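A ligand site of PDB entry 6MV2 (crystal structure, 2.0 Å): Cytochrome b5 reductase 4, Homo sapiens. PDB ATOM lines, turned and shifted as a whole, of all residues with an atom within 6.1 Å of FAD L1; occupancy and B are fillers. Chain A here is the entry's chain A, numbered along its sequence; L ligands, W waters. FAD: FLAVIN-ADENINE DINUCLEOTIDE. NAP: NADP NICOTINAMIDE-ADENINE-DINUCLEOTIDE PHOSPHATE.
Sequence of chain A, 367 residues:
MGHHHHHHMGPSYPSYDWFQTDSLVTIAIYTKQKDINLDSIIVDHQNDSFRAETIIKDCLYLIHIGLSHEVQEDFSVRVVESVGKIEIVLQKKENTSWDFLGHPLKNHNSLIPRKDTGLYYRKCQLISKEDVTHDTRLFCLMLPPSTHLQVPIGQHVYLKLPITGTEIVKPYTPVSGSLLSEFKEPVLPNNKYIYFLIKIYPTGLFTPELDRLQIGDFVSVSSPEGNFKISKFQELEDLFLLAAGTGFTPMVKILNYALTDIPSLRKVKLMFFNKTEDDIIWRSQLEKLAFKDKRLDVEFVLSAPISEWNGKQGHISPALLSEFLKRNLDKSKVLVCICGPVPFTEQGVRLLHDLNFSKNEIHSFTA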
ATOM      1  N   HIS A 156      27.066  -2.787  18.719  1.00  0.00           N
ATOM      2  CA  HIS A 156      26.279  -3.212  17.570  1.00  0.00           C
ATOM      3  C   HIS A 156      27.203  -3.807  16.509  1.00  0.00           C
ATOM      4  O   HIS A 156      28.427  -3.716  16.616  1.00  0.00           O
ATOM      5  CB  HIS A 156      25.499  -2.030  16.985  1.00  0.00           C
ATOM      6  CG  HIS A 156      26.328  -0.794  16.778  1.00  0.00           C
ATOM      7  ND1 HIS A 156      26.573   0.112  17.785  1.00  0.00           N
ATOM      8  CD2 HIS A 156      26.945  -0.314  15.677  1.00  0.00           C
ATOM      9  CE1 HIS A 156      27.327   1.090  17.324  1.00  0.00           C
ATOM     10  NE2 HIS A 156      27.559   0.861  16.038  1.00  0.00           N
ATOM     11  N   LYS A 170      23.050  -1.852   7.323  1.00  0.00           N
ATOM     12  CA  LYS A 170      22.490  -1.116   8.453  1.00  0.00           C
ATOM     13  C   LYS A 170      23.009  -1.732   9.754  1.00  0.00           C
ATOM     14  O   LYS A 170      23.304  -2.937   9.784  1.00  0.00           O
ATOM     15  CB  LYS A 170      20.947  -1.127   8.474  1.00  0.00           C
ATOM     16  CG  LYS A 170      20.281  -0.233   7.434  1.00  0.00           C
ATOM     17  CD  LYS A 170      20.433   1.213   7.830  1.00  0.00           C
ATOM     18  CE  LYS A 170      19.931   2.264   6.807  1.00  0.00           C
ATOM     19  NZ  LYS A 170      18.952   1.815   5.787  1.00  0.00           N
ATOM     20  N   PRO A 171      23.127  -0.948  10.824  1.00  0.00           N
ATOM     21  CA  PRO A 171      23.519  -1.495  12.134  1.00  0.00           C
ATOM     22  C   PRO A 171      22.360  -2.006  12.974  1.00  0.00           C
ATOM     23  O   PRO A 171      21.231  -1.494  12.947  1.00  0.00           O
ATOM     24  CB  PRO A 171      24.180  -0.276  12.822  1.00  0.00           C
ATOM     25  CG  PRO A 171      23.421   0.900  12.286  1.00  0.00           C
ATOM     26  CD  PRO A 171      23.061   0.526  10.847  1.00  0.00           C
ATOM     27  N   TYR A 172      22.647  -3.071  13.723  1.00  0.00           N
ATOM     28  CA  TYR A 172      21.702  -3.662  14.657  1.00  0.00           C
ATOM     29  C   TYR A 172      22.453  -4.108  15.906  1.00  0.00           C
ATOM     30  O   TYR A 172      23.630  -4.503  15.847  1.00  0.00           O
ATOM     31  CB  TYR A 172      20.945  -4.805  14.017  1.00  0.00           C
ATOM     32  CG  TYR A 172      20.184  -4.345  12.797  1.00  0.00           C
ATOM     33  CD1 TYR A 172      18.924  -3.802  12.914  1.00  0.00           C
ATOM     34  CD2 TYR A 172      20.749  -4.406  11.530  1.00  0.00           C
ATOM     35  CE1 TYR A 172      18.236  -3.328  11.818  1.00  0.00           C
ATOM     36  CE2 TYR A 172      20.065  -3.971  10.424  1.00  0.00           C
ATOM     37  CZ  TYR A 172      18.800  -3.420  10.585  1.00  0.00           C
ATOM     38  OH  TYR A 172      18.114  -2.953   9.518  1.00  0.00           O
ATOM     39  N   THR A 173      21.743  -4.070  17.027  1.00  0.00           N
ATOM     40  CA  THR A 173      22.332  -4.280  18.337  1.00  0.00           C
ATOM     41  C   THR A 173      22.003  -5.659  18.880  1.00  0.00           C
ATOM     42  O   THR A 173      20.869  -5.873  19.337  1.00  0.00           O
ATOM     43  CB  THR A 173      21.825  -3.221  19.294  1.00  0.00           C
ATOM     44  OG1 THR A 173      22.122  -1.936  18.771  1.00  0.00           O
ATOM     45  CG2 THR A 173      22.493  -3.383  20.682  1.00  0.00           C
ATOM     46  N   PRO A 174      22.941  -6.607  18.898  1.00  0.00           N
ATOM     47  CA  PRO A 174      22.607  -7.953  19.383  1.00  0.00           C
ATOM     48  C   PRO A 174      21.993  -7.931  20.780  1.00  0.00           C
ATOM     49  O   PRO A 174      22.336  -7.101  21.628  1.00  0.00           O
ATOM     50  CB  PRO A 174      23.949  -8.667  19.367  1.00  0.00           C
ATOM     51  CG  PRO A 174      24.630  -8.062  18.185  1.00  0.00           C
ATOM     52  CD  PRO A 174      24.271  -6.588  18.275  1.00  0.00           C
ATOM     53  N   VAL A 175      21.089  -8.880  20.989  1.00  0.00           N
ATOM     54  CA  VAL A 175      20.367  -9.027  22.235  1.00  0.00           C
ATOM     55  C   VAL A 175      20.580 -10.454  22.728  1.00  0.00           C
ATOM     56  O   VAL A 175      21.073 -11.320  22.008  1.00  0.00           O
ATOM     57  CB  VAL A 175      18.861  -8.752  22.059  1.00  0.00           C
ATOM     58  CG1 VAL A 175      18.639  -7.311  21.594  1.00  0.00           C
ATOM     59  CG2 VAL A 175      18.258  -9.725  21.030  1.00  0.00           C
ATOM     60  N   PHE A 196      18.940 -10.901  17.353  1.00  0.00           N
ATOM     61  CA  PHE A 196      18.549  -9.520  17.087  1.00  0.00           C
ATOM     62  C   PHE A 196      17.038  -9.380  17.183  1.00  0.00           C
ATOM     63  O   PHE A 196      16.302 -10.262  16.730  1.00  0.00           O
ATOM     64  CB  PHE A 196      18.954  -9.058  15.690  1.00  0.00           C
ATOM     65  CG  PHE A 196      20.415  -9.227  15.379  1.00  0.00           C
ATOM     66  CD1 PHE A 196      20.914 -10.462  14.976  1.00  0.00           C
ATOM     67  CD2 PHE A 196      21.287  -8.150  15.476  1.00  0.00           C
ATOM     68  CE1 PHE A 196      22.263 -10.596  14.681  1.00  0.00           C
ATOM     69  CE2 PHE A 196      22.606  -8.277  15.182  1.00  0.00           C
ATOM     70  CZ  PHE A 196      23.100  -9.478  14.781  1.00  0.00           C
ATOM     71  N   LEU A 197      16.589  -8.264  17.742  1.00  0.00           N
ATOM     72  CA  LEU A 197      15.205  -7.800  17.641  1.00  0.00           C
ATOM     73  C   LEU A 197      15.182  -6.704  16.613  1.00  0.00           C
ATOM     74  O   LEU A 197      15.833  -5.682  16.792  1.00  0.00           O
ATOM     75  CB  LEU A 197      14.696  -7.269  18.985  1.00  0.00           C
ATOM     76  CG  LEU A 197      14.556  -8.378  20.034  1.00  0.00           C
ATOM     77  CD1 LEU A 197      14.455  -7.758  21.440  1.00  0.00           C
ATOM     78  CD2 LEU A 197      13.307  -9.214  19.711  1.00  0.00           C
ATOM     79  N   ILE A 198      14.482  -6.914  15.502  1.00  0.00           N
ATOM     80  CA  ILE A 198      14.530  -6.000  14.379  1.00  0.00           C
ATOM     81  C   ILE A 198      13.117  -5.711  13.914  1.00  0.00           C
ATOM     82  O   ILE A 198      12.351  -6.636  13.603  1.00  0.00           O
ATOM     83  CB  ILE A 198      15.379  -6.559  13.220  1.00  0.00           C
ATOM     84  CG1 ILE A 198      16.834  -6.701  13.653  1.00  0.00           C
ATOM     85  CG2 ILE A 198      15.294  -5.634  11.988  1.00  0.00           C
ATOM     86  CD1 ILE A 198      17.743  -7.358  12.611  1.00  0.00           C
ATOM     87  N   LYS A 199      12.791  -4.445  13.859  1.00  0.00           N
ATOM     88  CA  LYS A 199      11.494  -3.959  13.415  1.00  0.00           C
ATOM     89  C   LYS A 199      11.556  -3.807  11.901  1.00  0.00           C
ATOM     90  O   LYS A 199      12.520  -3.256  11.366  1.00  0.00           O
ATOM     91  CB  LYS A 199      11.188  -2.620  14.095  1.00  0.00           C
ATOM     92  CG  LYS A 199       9.835  -1.969  13.683  1.00  0.00           C
ATOM     93  CD  LYS A 199       9.436  -0.743  14.562  1.00  0.00           C
ATOM     94  CE  LYS A 199       9.101  -1.161  15.967  1.00  0.00           C
ATOM     95  NZ  LYS A 199       8.677  -0.026  16.836  1.00  0.00           N
ATOM     96  N   ILE A 200      10.535  -4.325  11.224  1.00  0.00           N
ATOM     97  CA  ILE A 200      10.449  -4.273   9.763  1.00  0.00           C
ATOM     98  C   ILE A 200       9.569  -3.094   9.364  1.00  0.00           C
ATOM     99  O   ILE A 200       8.388  -3.018   9.757  1.00  0.00           O
ATOM    100  CB  ILE A 200       9.915  -5.598   9.187  1.00  0.00           C
ATOM    101  CG1 ILE A 200      10.632  -6.826   9.786  1.00  0.00           C
ATOM    102  CG2 ILE A 200       9.966  -5.604   7.646  1.00  0.00           C
ATOM    103  CD1 ILE A 200      12.198  -6.817   9.765  1.00  0.00           C
ATOM    104  N   TYR A 201      10.129  -2.174   8.572  1.00  0.00           N
ATOM    105  CA  TYR A 201       9.419  -1.022   8.070  1.00  0.00           C
ATOM    106  C   TYR A 201       9.005  -1.288   6.626  1.00  0.00           C
ATOM    107  O   TYR A 201       9.878  -1.394   5.756  1.00  0.00           O
ATOM    108  CB  TYR A 201      10.295   0.215   8.133  1.00  0.00           C
ATOM    109  CG  TYR A 201      10.766   0.567   9.535  1.00  0.00           C
ATOM    110  CD1 TYR A 201      10.000   1.367  10.388  1.00  0.00           C
ATOM    111  CD2 TYR A 201      11.976   0.078  10.006  1.00  0.00           C
ATOM    112  CE1 TYR A 201      10.447   1.694  11.677  1.00  0.00           C
ATOM    113  CE2 TYR A 201      12.430   0.394  11.288  1.00  0.00           C
ATOM    114  CZ  TYR A 201      11.662   1.203  12.112  1.00  0.00           C
ATOM    115  OH  TYR A 201      12.133   1.504  13.391  1.00  0.00           O
ATOM    116  N   THR A 203       8.166   0.525   4.264  1.00  0.00           N
ATOM    117  CA  THR A 203       8.733   1.484   3.323  1.00  0.00           C
ATOM    118  C   THR A 203      10.240   1.605   3.430  1.00  0.00           C
ATOM    119  O   THR A 203      10.825   2.467   2.757  1.00  0.00           O
ATOM    120  CB  THR A 203       8.072   2.868   3.506  1.00  0.00           C
ATOM    121  OG1 THR A 203       8.255   3.328   4.855  1.00  0.00           O
ATOM    122  CG2 THR A 203       6.597   2.775   3.220  1.00  0.00           C
ATOM    123  N   GLY A 204      10.896   0.742   4.219  1.00  0.00           N
ATOM    124  CA  GLY A 204      12.321   0.852   4.405  1.00  0.00           C
ATOM    125  C   GLY A 204      13.068   0.232   3.242  1.00  0.00           C
ATOM    126  O   GLY A 204      12.497  -0.426   2.385  1.00  0.00           O
ATOM    127  N   LEU A 205      14.388   0.451   3.226  1.00  0.00           N
ATOM    128  CA  LEU A 205      15.233  -0.201   2.226  1.00  0.00           C
ATOM    129  C   LEU A 205      15.755  -1.559   2.700  1.00  0.00           C
ATOM    130  O   LEU A 205      15.578  -2.575   2.010  1.00  0.00           O
ATOM    131  CB  LEU A 205      16.414   0.719   1.898  1.00  0.00           C
ATOM    132  CG  LEU A 205      17.434   0.133   0.900  1.00  0.00           C
ATOM    133  CD1 LEU A 205      16.773  -0.206  -0.397  1.00  0.00           C
ATOM    134  CD2 LEU A 205      18.523   1.126   0.695  1.00  0.00           C
ATOM    135  N   PHE A 206      16.372  -1.599   3.880  1.00  0.00           N
ATOM    136  CA  PHE A 206      17.060  -2.804   4.349  1.00  0.00           C
ATOM    137  C   PHE A 206      16.102  -3.816   4.971  1.00  0.00           C
ATOM    138  O   PHE A 206      16.123  -4.999   4.605  1.00  0.00           O
ATOM    139  CB  PHE A 206      18.141  -2.405   5.362  1.00  0.00           C
ATOM    140  CG  PHE A 206      19.071  -3.551   5.719  1.00  0.00           C
ATOM    141  CD1 PHE A 206      20.213  -3.791   4.982  1.00  0.00           C
ATOM    142  CD2 PHE A 206      18.773  -4.397   6.773  1.00  0.00           C
ATOM    143  CE1 PHE A 206      21.052  -4.848   5.293  1.00  0.00           C
ATOM    144  CE2 PHE A 206      19.599  -5.451   7.097  1.00  0.00           C
ATOM    145  CZ  PHE A 206      20.736  -5.685   6.344  1.00  0.00           C
ATOM    146  N   THR A 207      15.205  -3.387   5.861  1.00  0.00           N
ATOM    147  CA  THR A 207      14.485  -4.421   6.619  1.00  0.00           C
ATOM    148  C   THR A 207      13.510  -5.254   5.782  1.00  0.00           C
ATOM    149  O   THR A 207      13.319  -6.429   6.096  1.00  0.00           O
ATOM    150  CB  THR A 207      13.781  -3.809   7.831  1.00  0.00           C
ATOM    151  OG1 THR A 207      13.017  -2.662   7.460  1.00  0.00           O
ATOM    152  CG2 THR A 207      14.836  -3.393   8.897  1.00  0.00           C
ATOM    153  N   PRO A 208      12.858  -4.715   4.747  1.00  0.00           N
ATOM    154  CA  PRO A 208      12.076  -5.612   3.875  1.00  0.00           C
ATOM    155  C   PRO A 208      12.910  -6.684   3.204  1.00  0.00           C
ATOM    156  O   PRO A 208      12.416  -7.797   2.978  1.00  0.00           O
ATOM    157  CB  PRO A 208      11.464  -4.659   2.849  1.00  0.00           C
ATOM    158  CG  PRO A 208      11.442  -3.332   3.531  1.00  0.00           C
ATOM    159  CD  PRO A 208      12.687  -3.313   4.373  1.00  0.00           C
ATOM    160  N   GLU A 225      31.074  -2.683  16.986  1.00  0.00           N
ATOM    161  CA  GLU A 225      31.386  -1.259  17.070  1.00  0.00           C
ATOM    162  C   GLU A 225      30.610  -0.668  18.244  1.00  0.00           C
ATOM    163  O   GLU A 225      29.532  -1.154  18.608  1.00  0.00           O
ATOM    164  CB  GLU A 225      31.024  -0.532  15.757  1.00  0.00           C
ATOM    165  CG  GLU A 225      30.973   0.992  15.840  1.00  0.00           C
ATOM    166  CD  GLU A 225      30.515   1.658  14.546  1.00  0.00           C
ATOM    167  OE1 GLU A 225      29.329   2.121  14.440  1.00  0.00           O
ATOM    168  OE2 GLU A 225      31.346   1.730  13.624  1.00  0.00           O
ATOM    169  N   THR A 246      12.477   0.292  19.252  1.00  0.00           N
ATOM    170  CA  THR A 246      13.617  -0.617  19.189  1.00  0.00           C
ATOM    171  C   THR A 246      14.820  -0.096  19.946  1.00  0.00           C
ATOM    172  O   THR A 246      15.837  -0.793  19.967  1.00  0.00           O
ATOM    173  CB  THR A 246      14.035  -0.891  17.736  1.00  0.00           C
ATOM    174  OG1 THR A 246      14.562   0.308  17.163  1.00  0.00           O
ATOM    175  CG2 THR A 246      12.871  -1.377  16.890  1.00  0.00           C
ATOM    176  N   THR A 249      16.664  -2.479  22.332  1.00  0.00           N
ATOM    177  CA  THR A 249      17.607  -3.581  22.100  1.00  0.00           C
ATOM    178  C   THR A 249      18.921  -3.491  22.909  1.00  0.00           C
ATOM    179  O   THR A 249      19.326  -4.516  23.482  1.00  0.00           O
ATOM    180  CB  THR A 249      17.864  -3.782  20.611  1.00  0.00           C
ATOM    181  OG1 THR A 249      18.490  -2.649  20.006  1.00  0.00           O
ATOM    182  CG2 THR A 249      16.530  -4.075  19.915  1.00  0.00           C
ATOM    183  N   PRO A 250      19.650  -2.364  22.995  1.00  0.00           N
ATOM    184  CA  PRO A 250      20.847  -2.368  23.895  1.00  0.00           C
ATOM    185  C   PRO A 250      20.512  -2.647  25.329  1.00  0.00           C
ATOM    186  O   PRO A 250      21.379  -3.115  26.092  1.00  0.00           O
ATOM    187  CB  PRO A 250      21.439  -0.953  23.737  1.00  0.00           C
ATOM    188  CG  PRO A 250      20.331  -0.125  23.123  1.00  0.00           C
ATOM    189  CD  PRO A 250      19.527  -1.074  22.276  1.00  0.00           C
ATOM    190  N   THR A 366      23.694   5.846  20.490  1.00  0.00           N
ATOM    191  CA  THR A 366      23.454   6.513  19.211  1.00  0.00           C
ATOM    192  C   THR A 366      24.374   5.875  18.167  1.00  0.00           C
ATOM    193  O   THR A 366      25.064   4.887  18.430  1.00  0.00           O
ATOM    194  CB  THR A 366      23.676   8.026  19.346  1.00  0.00           C
ATOM    195  OG1 THR A 366      24.981   8.270  19.896  1.00  0.00           O
ATOM    196  CG2 THR A 366      22.615   8.642  20.232  1.00  0.00           C
ATOM    197  N   ALA A 367      24.406   6.457  16.976  1.00  0.00           N
ATOM    198  CA  ALA A 367      25.224   5.895  15.896  1.00  0.00           C
ATOM    199  C   ALA A 367      26.711   6.022  16.219  1.00  0.00           C
ATOM    200  O   ALA A 367      27.421   5.020  16.295  1.00  0.00           O
ATOM    201  CB  ALA A 367      24.915   6.584  14.564  1.00  0.00           C
HETATM  202  PA  FAD L   1      14.867   3.174   6.220  1.00  0.00           P
HETATM  203  O1A FAD L   1      14.964   3.079   4.720  1.00  0.00           O
HETATM  204  O2A FAD L   1      16.092   3.797   6.809  1.00  0.00           O
HETATM  205  O5B FAD L   1      13.583   4.022   6.635  1.00  0.00           O
HETATM  206  C5B FAD L   1      12.454   3.385   7.227  1.00  0.00           C
HETATM  207  C4B FAD L   1      11.238   4.299   7.225  1.00  0.00           C
HETATM  208  O4B FAD L   1      11.219   5.055   8.431  1.00  0.00           O
HETATM  209  C3B FAD L   1      11.200   5.329   6.098  1.00  0.00           C
HETATM  210  O3B FAD L   1      10.546   4.861   4.922  1.00  0.00           O
HETATM  211  C2B FAD L   1      10.429   6.459   6.733  1.00  0.00           C
HETATM  212  O2B FAD L   1       9.011   6.178   6.671  1.00  0.00           O
HETATM  213  C1B FAD L   1      10.972   6.440   8.153  1.00  0.00           C
HETATM  214  N9A FAD L   1      12.226   7.274   8.234  1.00  0.00           N
HETATM  215  C8A FAD L   1      13.475   6.935   7.825  1.00  0.00           C
HETATM  216  N7A FAD L   1      14.365   7.924   8.050  1.00  0.00           N
HETATM  217  C5A FAD L   1      13.694   8.937   8.627  1.00  0.00           C
HETATM  218  C6A FAD L   1      14.048  10.283   9.119  1.00  0.00           C
HETATM  219  N6A FAD L   1      15.320  10.749   9.042  1.00  0.00           N
HETATM  220  N1A FAD L   1      13.048  11.031   9.631  1.00  0.00           N
HETATM  221  C2A FAD L   1      11.784  10.582   9.719  1.00  0.00           C
HETATM  222  N3A FAD L   1      11.403   9.362   9.291  1.00  0.00           N
HETATM  223  C4A FAD L   1      12.292   8.502   8.738  1.00  0.00           C
HETATM  224  N1  FAD L   1      16.889  -1.242  14.493  1.00  0.00           N
HETATM  225  C2  FAD L   1      16.339  -2.363  14.994  1.00  0.00           C
HETATM  226  O2  FAD L   1      15.230  -2.746  14.579  1.00  0.00           O
HETATM  227  N3  FAD L   1      16.975  -3.097  15.932  1.00  0.00           N
HETATM  228  C4  FAD L   1      18.167  -2.797  16.449  1.00  0.00           C
HETATM  229  O4  FAD L   1      18.712  -3.521  17.297  1.00  0.00           O
HETATM  230  C4X FAD L   1      18.842  -1.589  15.969  1.00  0.00           C
HETATM  231  N5  FAD L   1      20.053  -1.206  16.441  1.00  0.00           N
HETATM  232  C5X FAD L   1      20.606  -0.061  15.936  1.00  0.00           C
HETATM  233  C6  FAD L   1      21.845   0.354  16.419  1.00  0.00           C
HETATM  234  C7  FAD L   1      22.454   1.506  15.937  1.00  0.00           C
HETATM  235  C7M FAD L   1      23.824   1.925  16.470  1.00  0.00           C
HETATM  236  C8  FAD L   1      21.752   2.341  14.918  1.00  0.00           C
HETATM  237  C8M FAD L   1      22.374   3.598  14.376  1.00  0.00           C
HETATM  238  C9  FAD L   1      20.499   1.937  14.417  1.00  0.00           C
HETATM  239  C9A FAD L   1      19.897   0.775  14.893  1.00  0.00           C
HETATM  240  N10 FAD L   1      18.640   0.351  14.419  1.00  0.00           N
HETATM  241  C10 FAD L   1      18.096  -0.812  14.947  1.00  0.00           C
HETATM  242  C1' FAD L   1      17.889   1.037  13.349  1.00  0.00           C
HETATM  243  C2' FAD L   1      18.402   0.331  12.084  1.00  0.00           C
HETATM  244  O2' FAD L   1      19.801   0.548  11.912  1.00  0.00           O
HETATM  245  C3' FAD L   1      17.795   0.820  10.761  1.00  0.00           C
HETATM  246  O3' FAD L   1      17.833   2.238  10.695  1.00  0.00           O
HETATM  247  C4' FAD L   1      16.364   0.361  10.626  1.00  0.00           C
HETATM  248  O4' FAD L   1      16.424  -1.058  10.556  1.00  0.00           O
HETATM  249  C5' FAD L   1      15.678   0.973   9.390  1.00  0.00           C
HETATM  250  O5' FAD L   1      16.396   0.654   8.212  1.00  0.00           O
HETATM  251  P   FAD L   1      15.606   0.466   6.821  1.00  0.00           P
HETATM  252  O1P FAD L   1      16.532   0.573   5.656  1.00  0.00           O
HETATM  253  O2P FAD L   1      14.787  -0.776   6.862  1.00  0.00           O
HETATM  254  O3P FAD L   1      14.553   1.700   6.823  1.00  0.00           O
HETATM  255  PA  NAP L   2       8.533   4.112  17.229  1.00  0.00           P
HETATM  256  O1A NAP L   2       7.715   2.902  17.611  1.00  0.00           O
HETATM  257  O2A NAP L   2       8.116   4.771  15.945  1.00  0.00           O
HETATM  258  O5B NAP L   2       8.346   5.172  18.428  1.00  0.00           O
HETATM  259  C5B NAP L   2       8.708   4.760  19.736  1.00  0.00           C
HETATM  260  C4B NAP L   2       8.176   5.772  20.741  1.00  0.00           C
HETATM  261  O4B NAP L   2       9.019   6.926  20.742  1.00  0.00           O
HETATM  262  C3B NAP L   2       6.757   6.246  20.395  1.00  0.00           C
HETATM  263  O3B NAP L   2       5.987   6.211  21.611  1.00  0.00           O
HETATM  264  C2B NAP L   2       6.977   7.626  19.772  1.00  0.00           C
HETATM  265  O2B NAP L   2       5.913   8.597  19.854  1.00  0.00           O
HETATM  266  C1B NAP L   2       8.204   8.086  20.529  1.00  0.00           C
HETATM  267  N9A NAP L   2       8.912   9.136  19.761  1.00  0.00           N
HETATM  268  C8A NAP L   2       9.289   9.102  18.469  1.00  0.00           C
HETATM  269  N7A NAP L   2       9.919  10.260  18.126  1.00  0.00           N
HETATM  270  C5A NAP L   2       9.934  11.034  19.218  1.00  0.00           C
HETATM  271  C6A NAP L   2      10.427  12.380  19.556  1.00  0.00           C
HETATM  272  N6A NAP L   2      11.049  13.147  18.626  1.00  0.00           N
HETATM  273  N1A NAP L   2      10.231  12.820  20.830  1.00  0.00           N
HETATM  274  C2A NAP L   2       9.621  12.078  21.766  1.00  0.00           C
HETATM  275  N3A NAP L   2       9.143  10.839  21.523  1.00  0.00           N
HETATM  276  C4A NAP L   2       9.269  10.287  20.286  1.00  0.00           C
HETATM  277  O3  NAP L   2      10.123   3.871  17.320  1.00  0.00           O
HETATM  278  PN  NAP L   2      10.984   2.878  16.400  1.00  0.00           P
HETATM  279  O1N NAP L   2      10.372   2.868  15.010  1.00  0.00           O
HETATM  280  O2N NAP L   2      11.030   1.554  17.116  1.00  0.00           O
HETATM  281  O5D NAP L   2      12.454   3.494  16.267  1.00  0.00           O
HETATM  282  C5D NAP L   2      13.330   3.460  17.393  1.00  0.00           C
HETATM  283  C4D NAP L   2      14.618   4.199  17.024  1.00  0.00           C
HETATM  284  O4D NAP L   2      15.666   3.784  17.893  1.00  0.00           O
HETATM  285  C3D NAP L   2      15.137   3.954  15.609  1.00  0.00           C
HETATM  286  O3D NAP L   2      15.286   5.245  15.030  1.00  0.00           O
HETATM  287  C2D NAP L   2      16.489   3.302  15.755  1.00  0.00           C
HETATM  288  O2D NAP L   2      17.448   3.744  14.810  1.00  0.00           O
HETATM  289  C1D NAP L   2      16.903   3.739  17.157  1.00  0.00           C
HETATM  290  N1N NAP L   2      17.862   2.816  17.736  1.00  0.00           N
HETATM  291  C2N NAP L   2      19.107   3.261  17.944  1.00  0.00           C
HETATM  292  C3N NAP L   2      20.089   2.450  18.482  1.00  0.00           C
HETATM  293  C7N NAP L   2      21.451   3.059  18.673  1.00  0.00           C
HETATM  294  O7N NAP L   2      21.783   4.052  18.047  1.00  0.00           O
HETATM  295  N7N NAP L   2      22.256   2.527  19.559  1.00  0.00           N
HETATM  296  C4N NAP L   2      19.794   1.141  18.828  1.00  0.00           C
HETATM  297  C5N NAP L   2      18.519   0.634  18.605  1.00  0.00           C
HETATM  298  C6N NAP L   2      17.449   1.447  18.043  1.00  0.00           C
HETATM  299  P2B NAP L   2       4.892   8.851  18.615  1.00  0.00           P
HETATM  300  O1X NAP L   2       4.509  10.313  18.572  1.00  0.00           O
HETATM  301  O2X NAP L   2       5.468   8.463  17.274  1.00  0.00           O
HETATM  302  O3X NAP L   2       3.685   7.994  18.906  1.00  0.00           O
HETATM  303  O   HOH W   1      18.689  -6.160  17.675  1.00  0.00           O
HETATM  304  O   HOH W   2      15.863   3.796  12.277  1.00  0.00           O
HETATM  305  O   HOH W   3      17.703   4.141   4.367  1.00  0.00           O
HETATM  306  O   HOH W   4      14.556   0.646  14.397  1.00  0.00           O
HETATM  307  O   HOH W   5      14.545  -1.787  12.289  1.00  0.00           O
HETATM  308  O   HOH W   6      20.791   3.232  10.984  1.00  0.00           O
HETATM  309  O   HOH W   7      17.727   4.193   8.746  1.00  0.00           O
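O2P of FAD L1 sits at hydrogen-bond distance from N of Thr 207, 2.8 Å away. O2P of FAD L1 sits at hydrogen-bond distance from OG1 of Thr 207, at 2.7 Å. O of Pro 171 lies within hydrogen-bond range of O2' of FAD L1 (2.7 Å). An oxygen (O1P) of FAD L1 is in salt-bridge range of the side-chain amino group (NZ) of Lys 170 (2.7 Å). OH of Tyr 172 is in hydrogen-bond range of O4' of FAD L1 (2.7 Å). An oxygen (O3B) of FAD L1 lies within hydrogen-bond range of the backbone carbonyl oxygen of Thr 203. OG1 of Thr 203 lies within hydrogen-bond range of O3B of FAD L1. An oxygen (O1P) of FAD L1 lies within hydrogen-bond range of the backbone NH (N) of Phe 206, 2.8 Å away. The side-chain hydroxyl of Thr 249 sits at hydrogen-bond distance from an oxygen (O4) of FAD L1, 2.9 Å away. N3 of FAD L1 is in hydrogen-bond range of O of Leu 197 (3.0 Å). The backbone NH of Lys 199 sits at hydrogen-bond distance from an oxygen (O2) of FAD L1, 3.1 Å away. An oxygen (O1A) of FAD L1 sits at hydrogen-bond distance from the backbone NH of Leu 205, 3.1 Å away. An oxygen (O4) of FAD L1 is in hydrogen-bond range of the backbone NH (N) of Thr 173 (3.1 Å). The side-chain hydroxyl (OG1) of Thr 173 is in hydrogen-bond range of a nitrogen (N5) of FAD L1 (3.2 Å). The side-chain amino group of Lys 199 is in salt-bridge range of an oxygen (O2N) of NAP L2. N of Thr 246 sits at hydrogen-bond distance from O2N of NAP L2 (2.9 Å). OH of Tyr 201 lies within hydrogen-bond range of O1N of NAP L2, 2.8 Å away.
OG1 of Thr 207 is in hydrogen-bond range of N of Tyr 201, at 3.1 Å. The side-chain hydroxyl (OG1) of Thr 249 is in hydrogen-bond range of the backbone carbonyl oxygen (O) of Thr 246 (3.2 Å). NE2 of His 156 sits at hydrogen-bond distance from OE1 of Glu 225 (2.7 Å).
Water W5 bridges O2 of FAD L1 (2.6 Å) and O of Lys 199 (2.7 Å). Water W1 lies within hydrogen-bond range of O4 of FAD L1, O of Thr 173 and N of Leu 197. Water W3 bridges an oxygen (O2A) of FAD L1 and the side-chain amino group of Lys 170. Water W2 bridges O3' of FAD L1 (3.0 Å) and O2D of NAP L2 (3.0 Å). Water W4 lies within hydrogen-bond range of OH of Tyr 201, OG1 of Thr 246 and N1 of FAD L1.
ND1 of His 156 touches C7M of FAD L1, 3.5 Å away. Ile 198 touches FAD L1. Tyr 201 touches FAD L1. Gly 204 touches FAD L1 (CA to O3P, 3.4 Å). Thr 246 touches FAD L1 (CG2 to O2, 3.6 Å). Thr 366 touches FAD L1. CB of Ala 367 touches C8M of FAD L1 (3.9 Å). Hydrophobic or aromatic side chains within 4 Å of FAD L1: His 156, Pro 171, Tyr 172, Ile 198, Tyr 201, Leu 205, Phe 206 and Ala 367. 18 residues have an atom within 4 Å of FAD L1: His 156, Lys 170, Pro 171, Tyr 172, Thr 173, Leu 197, Ile 198, Lys 199, Tyr 201, Thr 203, Gly 204, Leu 205, Phe 206, Thr 207, Thr 246, Thr 249, Thr 366 and Ala 367.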
